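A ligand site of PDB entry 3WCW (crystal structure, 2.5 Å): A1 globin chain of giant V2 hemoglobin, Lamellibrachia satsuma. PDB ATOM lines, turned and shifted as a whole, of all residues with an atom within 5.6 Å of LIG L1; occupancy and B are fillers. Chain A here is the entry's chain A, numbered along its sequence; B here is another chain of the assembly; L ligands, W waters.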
ATOM      1  N   TRP A  32      -9.483 -15.387   1.394  1.00  0.00           N
ATOM      2  CA  TRP A  32     -10.621 -16.240   1.702  1.00  0.00           C
ATOM      3  C   TRP A  32     -10.510 -17.103   2.955  1.00  0.00           C
ATOM      4  O   TRP A  32     -11.524 -17.439   3.568  1.00  0.00           O
ATOM      5  CB  TRP A  32     -10.934 -17.085   0.488  1.00  0.00           C
ATOM      6  CG  TRP A  32     -11.612 -16.253  -0.537  1.00  0.00           C
ATOM      7  CD1 TRP A  32     -11.037 -15.627  -1.597  1.00  0.00           C
ATOM      8  CD2 TRP A  32     -12.991 -15.899  -0.554  1.00  0.00           C
ATOM      9  NE1 TRP A  32     -11.978 -14.907  -2.277  1.00  0.00           N
ATOM     10  CE2 TRP A  32     -13.186 -15.062  -1.659  1.00  0.00           C
ATOM     11  CE3 TRP A  32     -14.092 -16.221   0.262  1.00  0.00           C
ATOM     12  CZ2 TRP A  32     -14.450 -14.516  -1.985  1.00  0.00           C
ATOM     13  CZ3 TRP A  32     -15.342 -15.697  -0.055  1.00  0.00           C
ATOM     14  CH2 TRP A  32     -15.507 -14.846  -1.172  1.00  0.00           C
ATOM     15  N   ALA A  42     -20.407 -17.860   6.471  1.00  0.00           N
ATOM     16  CA  ALA A  42     -20.405 -17.346   5.118  1.00  0.00           C
ATOM     17  C   ALA A  42     -19.984 -18.413   4.102  1.00  0.00           C
ATOM     18  O   ALA A  42     -20.295 -18.314   2.914  1.00  0.00           O
ATOM     19  CB  ALA A  42     -19.495 -16.125   5.002  1.00  0.00           C
ATOM     20  N   LEU A  45     -22.525 -20.177   1.883  1.00  0.00           N
ATOM     21  CA  LEU A  45     -23.067 -19.373   0.773  1.00  0.00           C
ATOM     22  C   LEU A  45     -22.355 -19.690  -0.536  1.00  0.00           C
ATOM     23  O   LEU A  45     -22.809 -19.285  -1.597  1.00  0.00           O
ATOM     24  CB  LEU A  45     -22.898 -17.880   1.032  1.00  0.00           C
ATOM     25  CG  LEU A  45     -23.560 -17.269   2.277  1.00  0.00           C
ATOM     26  CD1 LEU A  45     -22.904 -15.940   2.580  1.00  0.00           C
ATOM     27  CD2 LEU A  45     -25.049 -17.130   2.042  1.00  0.00           C
ATOM     28  N   PHE A  46     -21.238 -20.401  -0.445  1.00  0.00           N
ATOM     29  CA  PHE A  46     -20.452 -20.702  -1.624  1.00  0.00           C
ATOM     30  C   PHE A  46     -20.406 -22.165  -2.054  1.00  0.00           C
ATOM     31  O   PHE A  46     -19.375 -22.633  -2.551  1.00  0.00           O
ATOM     32  CB  PHE A  46     -19.032 -20.192  -1.412  1.00  0.00           C
ATOM     33  CG  PHE A  46     -18.968 -18.717  -1.263  1.00  0.00           C
ATOM     34  CD1 PHE A  46     -18.935 -17.902  -2.391  1.00  0.00           C
ATOM     35  CD2 PHE A  46     -18.963 -18.129  -0.004  1.00  0.00           C
ATOM     36  CE1 PHE A  46     -18.889 -16.522  -2.262  1.00  0.00           C
ATOM     37  CE2 PHE A  46     -18.927 -16.755   0.144  1.00  0.00           C
ATOM     38  CZ  PHE A  46     -18.894 -15.940  -0.984  1.00  0.00           C
ATOM     39  N   SER A  48     -21.877 -23.331  -4.526  1.00  0.00           N
ATOM     40  CA  SER A  48     -21.849 -23.318  -5.986  1.00  0.00           C
ATOM     41  C   SER A  48     -20.432 -23.251  -6.565  1.00  0.00           C
ATOM     42  O   SER A  48     -20.257 -23.269  -7.786  1.00  0.00           O
ATOM     43  CB  SER A  48     -22.667 -22.143  -6.520  1.00  0.00           C
ATOM     44  OG  SER A  48     -22.194 -20.906  -5.988  1.00  0.00           O
ATOM     45  N   VAL A  49     -19.430 -23.169  -5.696  1.00  0.00           N
ATOM     46  CA  VAL A  49     -18.039 -23.106  -6.143  1.00  0.00           C
ATOM     47  C   VAL A  49     -17.197 -23.965  -5.198  1.00  0.00           C
ATOM     48  O   VAL A  49     -16.030 -23.678  -4.950  1.00  0.00           O
ATOM     49  CB  VAL A  49     -17.494 -21.631  -6.202  1.00  0.00           C
ATOM     50  CG1 VAL A  49     -18.065 -20.904  -7.420  1.00  0.00           C
ATOM     51  CG2 VAL A  49     -17.863 -20.870  -4.933  1.00  0.00           C
ATOM     52  N   HIS A  62     -12.971 -19.498  -8.393  1.00  0.00           N
ATOM     53  CA  HIS A  62     -13.756 -18.431  -7.794  1.00  0.00           C
ATOM     54  C   HIS A  62     -12.808 -17.413  -7.160  1.00  0.00           C
ATOM     55  O   HIS A  62     -13.014 -16.212  -7.322  1.00  0.00           O
ATOM     56  CB  HIS A  62     -14.695 -18.987  -6.726  1.00  0.00           C
ATOM     57  CG  HIS A  62     -15.403 -17.929  -5.953  1.00  0.00           C
ATOM     58  ND1 HIS A  62     -16.396 -17.156  -6.499  1.00  0.00           N
ATOM     59  CD2 HIS A  62     -15.225 -17.483  -4.684  1.00  0.00           C
ATOM     60  CE1 HIS A  62     -16.801 -16.266  -5.600  1.00  0.00           C
ATOM     61  NE2 HIS A  62     -16.107 -16.443  -4.488  1.00  0.00           N
ATOM     62  N   ARG A  65     -11.436 -15.201  -9.808  1.00  0.00           N
ATOM     63  CA  ARG A  65     -12.361 -14.231 -10.378  1.00  0.00           C
ATOM     64  C   ARG A  65     -12.593 -13.055  -9.440  1.00  0.00           C
ATOM     65  O   ARG A  65     -12.665 -11.915  -9.861  1.00  0.00           O
ATOM     66  CB  ARG A  65     -13.704 -14.895 -10.746  1.00  0.00           C
ATOM     67  CG  ARG A  65     -13.660 -15.728 -12.058  1.00  0.00           C
ATOM     68  CD  ARG A  65     -15.055 -16.199 -12.524  1.00  0.00           C
ATOM     69  NE  ARG A  65     -15.700 -17.101 -11.575  1.00  0.00           N
ATOM     70  CZ  ARG A  65     -15.511 -18.418 -11.525  1.00  0.00           C
ATOM     71  NH1 ARG A  65     -14.697 -19.027 -12.381  1.00  0.00           N
ATOM     72  NH2 ARG A  65     -16.132 -19.133 -10.597  1.00  0.00           N
ATOM     73  N   VAL A  66     -12.654 -13.353  -8.143  1.00  0.00           N
ATOM     74  CA  VAL A  66     -12.870 -12.327  -7.140  1.00  0.00           C
ATOM     75  C   VAL A  66     -11.703 -11.367  -7.004  1.00  0.00           C
ATOM     76  O   VAL A  66     -11.910 -10.163  -6.915  1.00  0.00           O
ATOM     77  CB  VAL A  66     -13.140 -12.944  -5.761  1.00  0.00           C
ATOM     78  CG1 VAL A  66     -13.343 -11.836  -4.734  1.00  0.00           C
ATOM     79  CG2 VAL A  66     -14.363 -13.863  -5.822  1.00  0.00           C
ATOM     80  N   GLY A  69     -11.346  -9.237  -9.974  1.00  0.00           N
ATOM     81  CA  GLY A  69     -12.347  -8.182  -9.914  1.00  0.00           C
ATOM     82  C   GLY A  69     -11.872  -7.031  -9.046  1.00  0.00           C
ATOM     83  O   GLY A  69     -12.131  -5.861  -9.324  1.00  0.00           O
ATOM     84  N   LEU A  70     -11.176  -7.358  -7.970  1.00  0.00           N
ATOM     85  CA  LEU A  70     -10.644  -6.324  -7.084  1.00  0.00           C
ATOM     86  C   LEU A  70      -9.624  -5.510  -7.854  1.00  0.00           C
ATOM     87  O   LEU A  70      -9.557  -4.284  -7.739  1.00  0.00           O
ATOM     88  CB  LEU A  70      -9.960  -6.956  -5.860  1.00  0.00           C
ATOM     89  CG  LEU A  70     -10.909  -7.374  -4.753  1.00  0.00           C
ATOM     90  CD1 LEU A  70     -10.143  -8.102  -3.644  1.00  0.00           C
ATOM     91  CD2 LEU A  70     -11.589  -6.119  -4.231  1.00  0.00           C
ATOM     92  N   ARG A  72      -9.263  -5.176 -11.330  1.00  0.00           N
ATOM     93  CA  ARG A  72      -9.822  -4.328 -12.396  1.00  0.00           C
ATOM     94  C   ARG A  72     -10.569  -3.125 -11.830  1.00  0.00           C
ATOM     95  O   ARG A  72     -10.497  -2.030 -12.385  1.00  0.00           O
ATOM     96  CB  ARG A  72     -10.730  -5.142 -13.325  1.00  0.00           C
ATOM     97  CG  ARG A  72     -12.074  -5.557 -12.760  1.00  0.00           C
ATOM     98  CD  ARG A  72     -12.778  -6.423 -13.786  1.00  0.00           C
ATOM     99  NE  ARG A  72     -14.217  -6.214 -13.753  1.00  0.00           N
ATOM    100  CZ  ARG A  72     -15.108  -7.123 -13.391  1.00  0.00           C
ATOM    101  NH1 ARG A  72     -14.714  -8.329 -13.029  1.00  0.00           N
ATOM    102  NH2 ARG A  72     -16.400  -6.826 -13.380  1.00  0.00           N
ATOM    103  N   LEU A  90     -21.049  -5.671 -11.397  1.00  0.00           N
ATOM    104  CA  LEU A  90     -20.842  -6.588 -10.288  1.00  0.00           C
ATOM    105  C   LEU A  90     -22.087  -6.622  -9.420  1.00  0.00           C
ATOM    106  O   LEU A  90     -22.453  -7.671  -8.893  1.00  0.00           O
ATOM    107  CB  LEU A  90     -19.636  -6.161  -9.432  1.00  0.00           C
ATOM    108  CG  LEU A  90     -18.273  -6.010 -10.128  1.00  0.00           C
ATOM    109  CD1 LEU A  90     -17.195  -5.547  -9.146  1.00  0.00           C
ATOM    110  CD2 LEU A  90     -17.912  -7.347 -10.726  1.00  0.00           C
ATOM    111  N   GLN A  93     -24.516  -8.956 -10.606  1.00  0.00           N
ATOM    112  CA  GLN A  93     -24.199 -10.347 -10.362  1.00  0.00           C
ATOM    113  C   GLN A  93     -24.393 -10.721  -8.896  1.00  0.00           C
ATOM    114  O   GLN A  93     -24.684 -11.871  -8.588  1.00  0.00           O
ATOM    115  CB  GLN A  93     -22.753 -10.662 -10.784  1.00  0.00           C
ATOM    116  CG  GLN A  93     -22.549 -10.571 -12.271  1.00  0.00           C
ATOM    117  CD  GLN A  93     -21.084 -10.537 -12.670  1.00  0.00           C
ATOM    118  OE1 GLN A  93     -20.322  -9.700 -12.186  1.00  0.00           O
ATOM    119  NE2 GLN A  93     -20.699 -11.440 -13.569  1.00  0.00           N
ATOM    120  N   HIS A  94     -24.260  -9.759  -7.986  1.00  0.00           N
ATOM    121  CA  HIS A  94     -24.447 -10.103  -6.585  1.00  0.00           C
ATOM    122  C   HIS A  94     -25.869  -9.949  -6.093  1.00  0.00           C
ATOM    123  O   HIS A  94     -26.282 -10.647  -5.173  1.00  0.00           O
ATOM    124  CB  HIS A  94     -23.489  -9.295  -5.706  1.00  0.00           C
ATOM    125  CG  HIS A  94     -22.061  -9.713  -5.845  1.00  0.00           C
ATOM    126  ND1 HIS A  94     -21.309  -9.420  -6.962  1.00  0.00           N
ATOM    127  CD2 HIS A  94     -21.242 -10.416  -5.024  1.00  0.00           C
ATOM    128  CE1 HIS A  94     -20.095  -9.911  -6.823  1.00  0.00           C
ATOM    129  NE2 HIS A  94     -20.020 -10.526  -5.651  1.00  0.00           N
ATOM    130  N   ARG A  97     -28.436 -12.882  -5.526  1.00  0.00           N
ATOM    131  CA  ARG A  97     -28.106 -13.852  -4.495  1.00  0.00           C
ATOM    132  C   ARG A  97     -28.557 -13.452  -3.102  1.00  0.00           C
ATOM    133  O   ARG A  97     -28.307 -14.190  -2.143  1.00  0.00           O
ATOM    134  CB  ARG A  97     -26.614 -14.173  -4.532  1.00  0.00           C
ATOM    135  CG  ARG A  97     -26.234 -14.806  -5.853  1.00  0.00           C
ATOM    136  CD  ARG A  97     -24.864 -15.409  -5.835  1.00  0.00           C
ATOM    137  NE  ARG A  97     -24.745 -16.454  -6.861  1.00  0.00           N
ATOM    138  CZ  ARG A  97     -24.374 -16.236  -8.127  1.00  0.00           C
ATOM    139  NH1 ARG A  97     -24.074 -15.009  -8.540  1.00  0.00           N
ATOM    140  NH2 ARG A  97     -24.311 -17.247  -8.970  1.00  0.00           N
ATOM    141  N   LEU A  99     -27.611 -11.382  -0.766  1.00  0.00           N
ATOM    142  CA  LEU A  99     -26.541 -11.453   0.208  1.00  0.00           C
ATOM    143  C   LEU A  99     -26.677 -10.393   1.293  1.00  0.00           C
ATOM    144  O   LEU A  99     -26.917  -9.216   1.022  1.00  0.00           O
ATOM    145  CB  LEU A  99     -25.186 -11.291  -0.493  1.00  0.00           C
ATOM    146  CG  LEU A  99     -24.855 -12.248  -1.635  1.00  0.00           C
ATOM    147  CD1 LEU A  99     -23.583 -11.768  -2.332  1.00  0.00           C
ATOM    148  CD2 LEU A  99     -24.684 -13.665  -1.111  1.00  0.00           C
ATOM    149  N   ASN A 103     -21.705  -9.209   5.321  1.00  0.00           N
ATOM    150  CA  ASN A 103     -20.606 -10.020   4.789  1.00  0.00           C
ATOM    151  C   ASN A 103     -19.604  -9.195   3.988  1.00  0.00           C
ATOM    152  O   ASN A 103     -18.422  -9.535   3.924  1.00  0.00           O
ATOM    153  CB  ASN A 103     -21.143 -11.177   3.962  1.00  0.00           C
ATOM    154  CG  ASN A 103     -21.674 -12.300   4.831  1.00  0.00           C
ATOM    155  OD1 ASN A 103     -22.597 -13.006   4.455  1.00  0.00           O
ATOM    156  ND2 ASN A 103     -21.075 -12.469   6.004  1.00  0.00           N
ATOM    157  N   PHE A 104     -20.077  -8.125   3.356  1.00  0.00           N
ATOM    158  CA  PHE A 104     -19.194  -7.253   2.617  1.00  0.00           C
ATOM    159  C   PHE A 104     -18.300  -6.533   3.637  1.00  0.00           C
ATOM    160  O   PHE A 104     -17.145  -6.212   3.349  1.00  0.00           O
ATOM    161  CB  PHE A 104     -19.991  -6.253   1.781  1.00  0.00           C
ATOM    162  CG  PHE A 104     -20.525  -6.843   0.514  1.00  0.00           C
ATOM    163  CD1 PHE A 104     -19.782  -6.788  -0.655  1.00  0.00           C
ATOM    164  CD2 PHE A 104     -21.722  -7.563   0.515  1.00  0.00           C
ATOM    165  CE1 PHE A 104     -20.204  -7.445  -1.814  1.00  0.00           C
ATOM    166  CE2 PHE A 104     -22.160  -8.216  -0.630  1.00  0.00           C
ATOM    167  CZ  PHE A 104     -21.396  -8.166  -1.799  1.00  0.00           C
ATOM    168  N   PHE A 107     -15.727  -9.043   4.454  1.00  0.00           N
ATOM    169  CA  PHE A 107     -14.810  -9.085   3.316  1.00  0.00           C
ATOM    170  C   PHE A 107     -13.749  -7.983   3.461  1.00  0.00           C
ATOM    171  O   PHE A 107     -12.546  -8.245   3.356  1.00  0.00           O
ATOM    172  CB  PHE A 107     -15.595  -8.883   2.026  1.00  0.00           C
ATOM    173  CG  PHE A 107     -14.791  -9.112   0.777  1.00  0.00           C
ATOM    174  CD1 PHE A 107     -13.931  -8.141   0.297  1.00  0.00           C
ATOM    175  CD2 PHE A 107     -14.927 -10.296   0.064  1.00  0.00           C
ATOM    176  CE1 PHE A 107     -13.199  -8.336  -0.870  1.00  0.00           C
ATOM    177  CE2 PHE A 107     -14.206 -10.504  -1.114  1.00  0.00           C
ATOM    178  CZ  PHE A 107     -13.334  -9.520  -1.584  1.00  0.00           C
ATOM    179  N   TYR A 132     -12.506   1.091   0.182  1.00  0.00           N
ATOM    180  CA  TYR A 132     -13.228  -0.165   0.102  1.00  0.00           C
ATOM    181  C   TYR A 132     -14.700   0.146   0.207  1.00  0.00           C
ATOM    182  O   TYR A 132     -15.527  -0.439  -0.508  1.00  0.00           O
ATOM    183  CB  TYR A 132     -12.838  -1.131   1.215  1.00  0.00           C
ATOM    184  CG  TYR A 132     -13.706  -2.381   1.201  1.00  0.00           C
ATOM    185  CD1 TYR A 132     -14.780  -2.529   2.086  1.00  0.00           C
ATOM    186  CD2 TYR A 132     -13.493  -3.385   0.252  1.00  0.00           C
ATOM    187  CE1 TYR A 132     -15.629  -3.638   2.016  1.00  0.00           C
ATOM    188  CE2 TYR A 132     -14.333  -4.487   0.163  1.00  0.00           C
ATOM    189  CZ  TYR A 132     -15.394  -4.616   1.050  1.00  0.00           C
ATOM    190  OH  TYR A 132     -16.212  -5.717   0.951  1.00  0.00           O
ATOM    191  N   ILE A 135     -16.078   0.687  -3.038  1.00  0.00           N
ATOM    192  CA  ILE A 135     -16.304  -0.521  -3.815  1.00  0.00           C
ATOM    193  C   ILE A 135     -17.576  -1.247  -3.387  1.00  0.00           C
ATOM    194  O   ILE A 135     -18.436  -1.555  -4.224  1.00  0.00           O
ATOM    195  CB  ILE A 135     -15.088  -1.485  -3.727  1.00  0.00           C
ATOM    196  CG1 ILE A 135     -13.910  -0.856  -4.496  1.00  0.00           C
ATOM    197  CG2 ILE A 135     -15.453  -2.863  -4.329  1.00  0.00           C
ATOM    198  CD1 ILE A 135     -12.567  -1.591  -4.365  1.00  0.00           C
ATOM    199  N   ALA A 136     -17.687  -1.479  -2.072  1.00  0.00           N
ATOM    200  CA  ALA A 136     -18.829  -2.145  -1.439  1.00  0.00           C
ATOM    201  C   ALA A 136     -20.120  -1.421  -1.773  1.00  0.00           C
ATOM    202  O   ALA A 136     -21.155  -2.033  -2.015  1.00  0.00           O
ATOM    203  CB  ALA A 136     -18.626  -2.186   0.081  1.00  0.00           C
ATOM    204  N   ILE A 139     -21.183  -2.253  -5.323  1.00  0.00           N
ATOM    205  CA  ILE A 139     -21.647  -3.608  -5.505  1.00  0.00           C
ATOM    206  C   ILE A 139     -22.962  -3.900  -4.810  1.00  0.00           C
ATOM    207  O   ILE A 139     -23.781  -4.637  -5.350  1.00  0.00           O
ATOM    208  CB  ILE A 139     -20.567  -4.639  -5.080  1.00  0.00           C
ATOM    209  CG1 ILE A 139     -19.283  -4.395  -5.875  1.00  0.00           C
ATOM    210  CG2 ILE A 139     -21.056  -6.065  -5.341  1.00  0.00           C
ATOM    211  CD1 ILE A 139     -18.158  -5.346  -5.561  1.00  0.00           C
ATOM    212  N   HIS B  94     -16.201 -21.718 -17.057  1.00  0.00           N
ATOM    213  CA  HIS B  94     -17.001 -20.582 -16.583  1.00  0.00           C
ATOM    214  C   HIS B  94     -17.091 -19.522 -17.689  1.00  0.00           C
ATOM    215  O   HIS B  94     -18.182 -19.043 -18.038  1.00  0.00           O
ATOM    216  CB  HIS B  94     -16.361 -19.949 -15.337  1.00  0.00           C
ATOM    217  CG  HIS B  94     -17.209 -18.894 -14.690  1.00  0.00           C
ATOM    218  ND1 HIS B  94     -18.215 -19.198 -13.790  1.00  0.00           N
ATOM    219  CD2 HIS B  94     -17.220 -17.549 -14.842  1.00  0.00           C
ATOM    220  CE1 HIS B  94     -18.806 -18.079 -13.424  1.00  0.00           C
ATOM    221  NE2 HIS B  94     -18.232 -17.060 -14.041  1.00  0.00           N
ATOM    222  N   GLN B  98     -20.292 -18.042 -19.969  1.00  0.00           N
ATOM    223  CA  GLN B  98     -20.595 -16.628 -20.120  1.00  0.00           C
ATOM    224  C   GLN B  98     -20.693 -16.202 -21.584  1.00  0.00           C
ATOM    225  O   GLN B  98     -21.226 -15.129 -21.895  1.00  0.00           O
ATOM    226  CB  GLN B  98     -19.546 -15.771 -19.409  1.00  0.00           C
ATOM    227  CG  GLN B  98     -19.539 -15.961 -17.891  1.00  0.00           C
ATOM    228  CD  GLN B  98     -18.438 -15.163 -17.207  1.00  0.00           C
ATOM    229  OE1 GLN B  98     -17.275 -15.275 -17.566  1.00  0.00           O
ATOM    230  NE2 GLN B  98     -18.813 -14.365 -16.211  1.00  0.00           N
HETATM  231  C1  LIG L   1     -19.200 -14.042  -7.524  1.00  0.00           C
HETATM  232  C2  LIG L   1     -16.424 -10.219  -7.027  1.00  0.00           C
HETATM  233  C3  LIG L   1     -17.778  -9.776  -2.436  1.00  0.00           C
HETATM  234  C4  LIG L   1     -20.612 -13.610  -2.971  1.00  0.00           C
HETATM  235  C5  LIG L   1     -18.307 -13.041  -7.805  1.00  0.00           C
HETATM  236  C6  LIG L   1     -17.683 -12.891  -9.050  1.00  0.00           C
HETATM  237  C7  LIG L   1     -16.890 -11.804  -8.926  1.00  0.00           C
HETATM  238  C8  LIG L   1     -17.037 -11.275  -7.574  1.00  0.00           C
HETATM  239  C9  LIG L   1     -15.982 -11.198  -9.998  1.00  0.00           C
HETATM  240  C10 LIG L   1     -17.857 -13.765 -10.273  1.00  0.00           C
HETATM  241  C11 LIG L   1     -18.858 -13.197 -11.247  1.00  0.00           C
HETATM  242  C12 LIG L   1     -19.059 -14.067 -12.482  1.00  0.00           C
HETATM  243  O1  LIG L   1     -20.178 -14.600 -12.684  1.00  0.00           O
HETATM  244  O2  LIG L   1     -18.125 -14.234 -13.212  1.00  0.00           O
HETATM  245  C13 LIG L   1     -16.534  -9.721  -5.720  1.00  0.00           C
HETATM  246  C14 LIG L   1     -15.805  -8.568  -5.229  1.00  0.00           C
HETATM  247  C15 LIG L   1     -16.218  -8.449  -3.853  1.00  0.00           C
HETATM  248  C16 LIG L   1     -17.137  -9.520  -3.652  1.00  0.00           C
HETATM  249  C17 LIG L   1     -14.848  -7.708  -5.982  1.00  0.00           C
HETATM  250  C18 LIG L   1     -15.724  -7.424  -2.953  1.00  0.00           C
HETATM  251  C19 LIG L   1     -16.062  -6.159  -2.980  1.00  0.00           C
HETATM  252  C20 LIG L   1     -18.671 -10.794  -2.193  1.00  0.00           C
HETATM  253  C21 LIG L   1     -19.301 -10.998  -0.876  1.00  0.00           C
HETATM  254  C22 LIG L   1     -20.144 -12.106  -0.995  1.00  0.00           C
HETATM  255  C23 LIG L   1     -19.970 -12.540  -2.436  1.00  0.00           C
HETATM  256  C24 LIG L   1     -19.066 -10.142   0.376  1.00  0.00           C
HETATM  257  C25 LIG L   1     -20.925 -12.666  -0.028  1.00  0.00           C
HETATM  258  C26 LIG L   1     -20.818 -13.514   0.937  1.00  0.00           C
HETATM  259  C27 LIG L   1     -20.485 -14.066  -4.270  1.00  0.00           C
HETATM  260  C28 LIG L   1     -21.218 -15.276  -4.805  1.00  0.00           C
HETATM  261  C29 LIG L   1     -20.794 -15.378  -6.116  1.00  0.00           C
HETATM  262  C30 LIG L   1     -19.845 -14.263  -6.346  1.00  0.00           C
HETATM  263  C31 LIG L   1     -22.183 -16.127  -3.994  1.00  0.00           C
HETATM  264  C32 LIG L   1     -21.196 -16.412  -7.153  1.00  0.00           C
HETATM  265  C33 LIG L   1     -20.313 -17.622  -7.163  1.00  0.00           C
HETATM  266  C34 LIG L   1     -20.691 -18.602  -8.195  1.00  0.00           C
HETATM  267  O3  LIG L   1     -21.385 -19.610  -7.903  1.00  0.00           O
HETATM  268  O4  LIG L   1     -20.297 -18.412  -9.356  1.00  0.00           O
HETATM  269  N1  LIG L   1     -17.920 -12.060  -6.883  1.00  0.00           N
HETATM  270  N2  LIG L   1     -17.327 -10.298  -4.818  1.00  0.00           N
HETATM  271  N3  LIG L   1     -19.107 -11.751  -3.088  1.00  0.00           N
HETATM  272  N4  LIG L   1     -19.699 -13.512  -5.215  1.00  0.00           N
HETATM  273 FE1  LIG L   1     -18.537 -11.904  -4.999  1.00  0.00          FE
HETATM  274  O1  LG2 L   2     -17.307 -13.099  -4.433  1.00  0.00           O
HETATM  275  O2  LG2 L   2     -17.269 -13.980  -3.561  1.00  0.00           O
HETATM  276  C1  LG3 L   3     -18.217 -10.832 -22.187  1.00  0.00           C
HETATM  277  C2  LG3 L   3     -13.718 -12.389 -21.937  1.00  0.00           C
HETATM  278  C3  LG3 L   3     -13.634 -13.121 -26.713  1.00  0.00           C
HETATM  279  C4  LG3 L   3     -18.203 -11.611 -26.941  1.00  0.00           C
HETATM  280  C5  LG3 L   3     -16.986 -11.192 -21.676  1.00  0.00           C
HETATM  281  C6  LG3 L   3     -16.651 -11.082 -20.319  1.00  0.00           C
HETATM  282  C7  LG3 L   3     -15.376 -11.532 -20.221  1.00  0.00           C
HETATM  283  C8  LG3 L   3     -14.911 -11.920 -21.566  1.00  0.00           C
HETATM  284  C9  LG3 L   3     -14.526 -11.624 -18.945  1.00  0.00           C
HETATM  285  C10 LG3 L   3     -17.518 -10.567 -19.189  1.00  0.00           C
HETATM  286  C11 LG3 L   3     -18.159 -11.635 -18.375  1.00  0.00           C
HETATM  287  C12 LG3 L   3     -19.035 -11.092 -17.249  1.00  0.00           C
HETATM  288  O1  LG3 L   3     -20.252 -10.914 -17.457  1.00  0.00           O
HETATM  289  O2  LG3 L   3     -18.523 -10.826 -16.210  1.00  0.00           O
HETATM  290  C13 LG3 L   3     -13.249 -12.742 -23.231  1.00  0.00           C
HETATM  291  C14 LG3 L   3     -11.904 -13.223 -23.511  1.00  0.00           C
HETATM  292  C15 LG3 L   3     -11.892 -13.426 -24.945  1.00  0.00           C
HETATM  293  C16 LG3 L   3     -13.205 -13.067 -25.377  1.00  0.00           C
HETATM  294  C17 LG3 L   3     -10.801 -13.442 -22.532  1.00  0.00           C
HETATM  295  C18 LG3 L   3     -10.727 -13.898 -25.670  1.00  0.00           C
HETATM  296  C19 LG3 L   3     -10.610 -15.099 -26.188  1.00  0.00           C
HETATM  297  C20 LG3 L   3     -14.892 -12.776 -27.174  1.00  0.00           C
HETATM  298  C21 LG3 L   3     -15.255 -12.863 -28.605  1.00  0.00           C
HETATM  299  C22 LG3 L   3     -16.597 -12.430 -28.721  1.00  0.00           C
HETATM  300  C23 LG3 L   3     -16.979 -12.089 -27.279  1.00  0.00           C
HETATM  301  C24 LG3 L   3     -14.328 -13.333 -29.722  1.00  0.00           C
HETATM  302  C25 LG3 L   3     -17.348 -12.338 -29.839  1.00  0.00           C
HETATM  303  C26 LG3 L   3     -17.585 -11.506 -30.790  1.00  0.00           C
HETATM  304  C27 LG3 L   3     -18.614 -11.258 -25.655  1.00  0.00           C
HETATM  305  C28 LG3 L   3     -19.992 -10.717 -25.333  1.00  0.00           C
HETATM  306  C29 LG3 L   3     -19.964 -10.499 -23.984  1.00  0.00           C
HETATM  307  C30 LG3 L   3     -18.626 -10.907 -23.500  1.00  0.00           C
HETATM  308  C31 LG3 L   3     -21.103 -10.481 -26.362  1.00  0.00           C
HETATM  309  C32 LG3 L   3     -21.089  -9.943 -23.132  1.00  0.00           C
HETATM  310  C33 LG3 L   3     -21.055  -8.435 -23.085  1.00  0.00           C
HETATM  311  C34 LG3 L   3     -22.135  -7.853 -22.258  1.00  0.00           C
HETATM  312  O3  LG3 L   3     -22.106  -7.975 -20.987  1.00  0.00           O
HETATM  313  O4  LG3 L   3     -23.075  -7.231 -22.838  1.00  0.00           O
HETATM  314  N1  LG3 L   3     -15.933 -11.707 -22.455  1.00  0.00           N
HETATM  315  N2  LG3 L   3     -14.028 -12.641 -24.308  1.00  0.00           N
HETATM  316  N3  LG3 L   3     -15.960 -12.307 -26.419  1.00  0.00           N
HETATM  317  N4  LG3 L   3     -17.856 -11.356 -24.540  1.00  0.00           N
HETATM  318 FE1  LG3 L   3     -15.950 -12.016 -24.432  1.00  0.00          FE
HETATM  319  O   HOH W   1     -17.646 -17.219  -9.159  1.00  0.00           O
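An oxygen (O2) of LG3 L3 lies within hydrogen-bond range of the side-chain amide nitrogen of Gln 93 (3.5 Å).
An iron atom (FE1) of LIG L1 is bound by a ring nitrogen (NE2) of His 94 of chain A (2.1 Å).
O3 of LIG L1 is in salt-bridge range of NH2 of Arg 97, at 3.9 Å.
NE2 of His 94 of chain B sits at hydrogen-bond distance from O2 of LIG L1 (2.9 Å).
A ring nitrogen (NE2) of His 62 lies within hydrogen-bond range of an oxygen (O2) of LG2 L2 (2.9 Å).
An oxygen (O1) of LIG L1 sits close to the side-chain amide nitrogen (NE2) of Gln 93 (3.3 Å).
An oxygen (O2) of LIG L1 is in hydrogen-bond range of the side-chain amide nitrogen (NE2) of Gln 98 of chain B (3.1 Å).
An oxygen (O3) of LIG L1 lies within hydrogen-bond range of the side-chain hydroxyl (OG) of Ser 48, 2.4 Å away.
An iron atom (FE1) of LIG L1 is bound by an oxygen (O1) of LG2 L2 (1.8 Å).
CD1 of Leu 45 touches C26 of LIG L1, at 3.6 Å.
CE1 of Phe 46 touches C4 of LIG L1, 3.5 Å away.
Val 49 touches LIG L1 (CG1 to C34, 3.6 Å).
CE1 of His 62 touches C30 of LIG L1, at 3.7 Å.
Arg 65 touches LIG L1.
O of Val 66 touches C17 of LIG L1 (3.9 Å).
Leu 99 touches LIG L1.
Asn 103 touches LIG L1 (O to C24, 3.7 Å).
Phe 104 touches LIG L1 (CE1 to C3, 3.4 Å).
Phe 107 touches LIG L1.
CE2 of Tyr 132 touches C19 of LIG L1 (3.96 Å).
Ile 135 touches LIG L1 (CG2 to C19, 3.6 Å).
Ile 139 touches LIG L1 (CD1 to C19, 3.4 Å).
Hydrophobic or aromatic side chains within 4 Å of LIG L1: Leu 45, Phe 46, Val 49, His 62, Val 66, His 94 of chain A, Leu 99, Phe 104, Phe 107, Tyr 132, Ile 135, Ile 139 and His 94 of chain B.
O of Gln 93 sits at hydrogen-bond distance from NH1 of Arg 97 (3.2 Å).
A ring nitrogen (ND1) of His 94 of chain A is in hydrogen-bond range of the backbone carbonyl oxygen (O) of Leu 90, 2.8 Å away.
OH of Tyr 132 sits at hydrogen-bond distance from O of Phe 104 (2.6 Å).
Water W1 lies within hydrogen-bond range of the guanidinium group (NH2) of Arg 65 (2.8 Å), an oxygen (O4) of LIG L1 (2.9 Å) and a ring nitrogen (ND1) of His 62 (2.9 Å).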
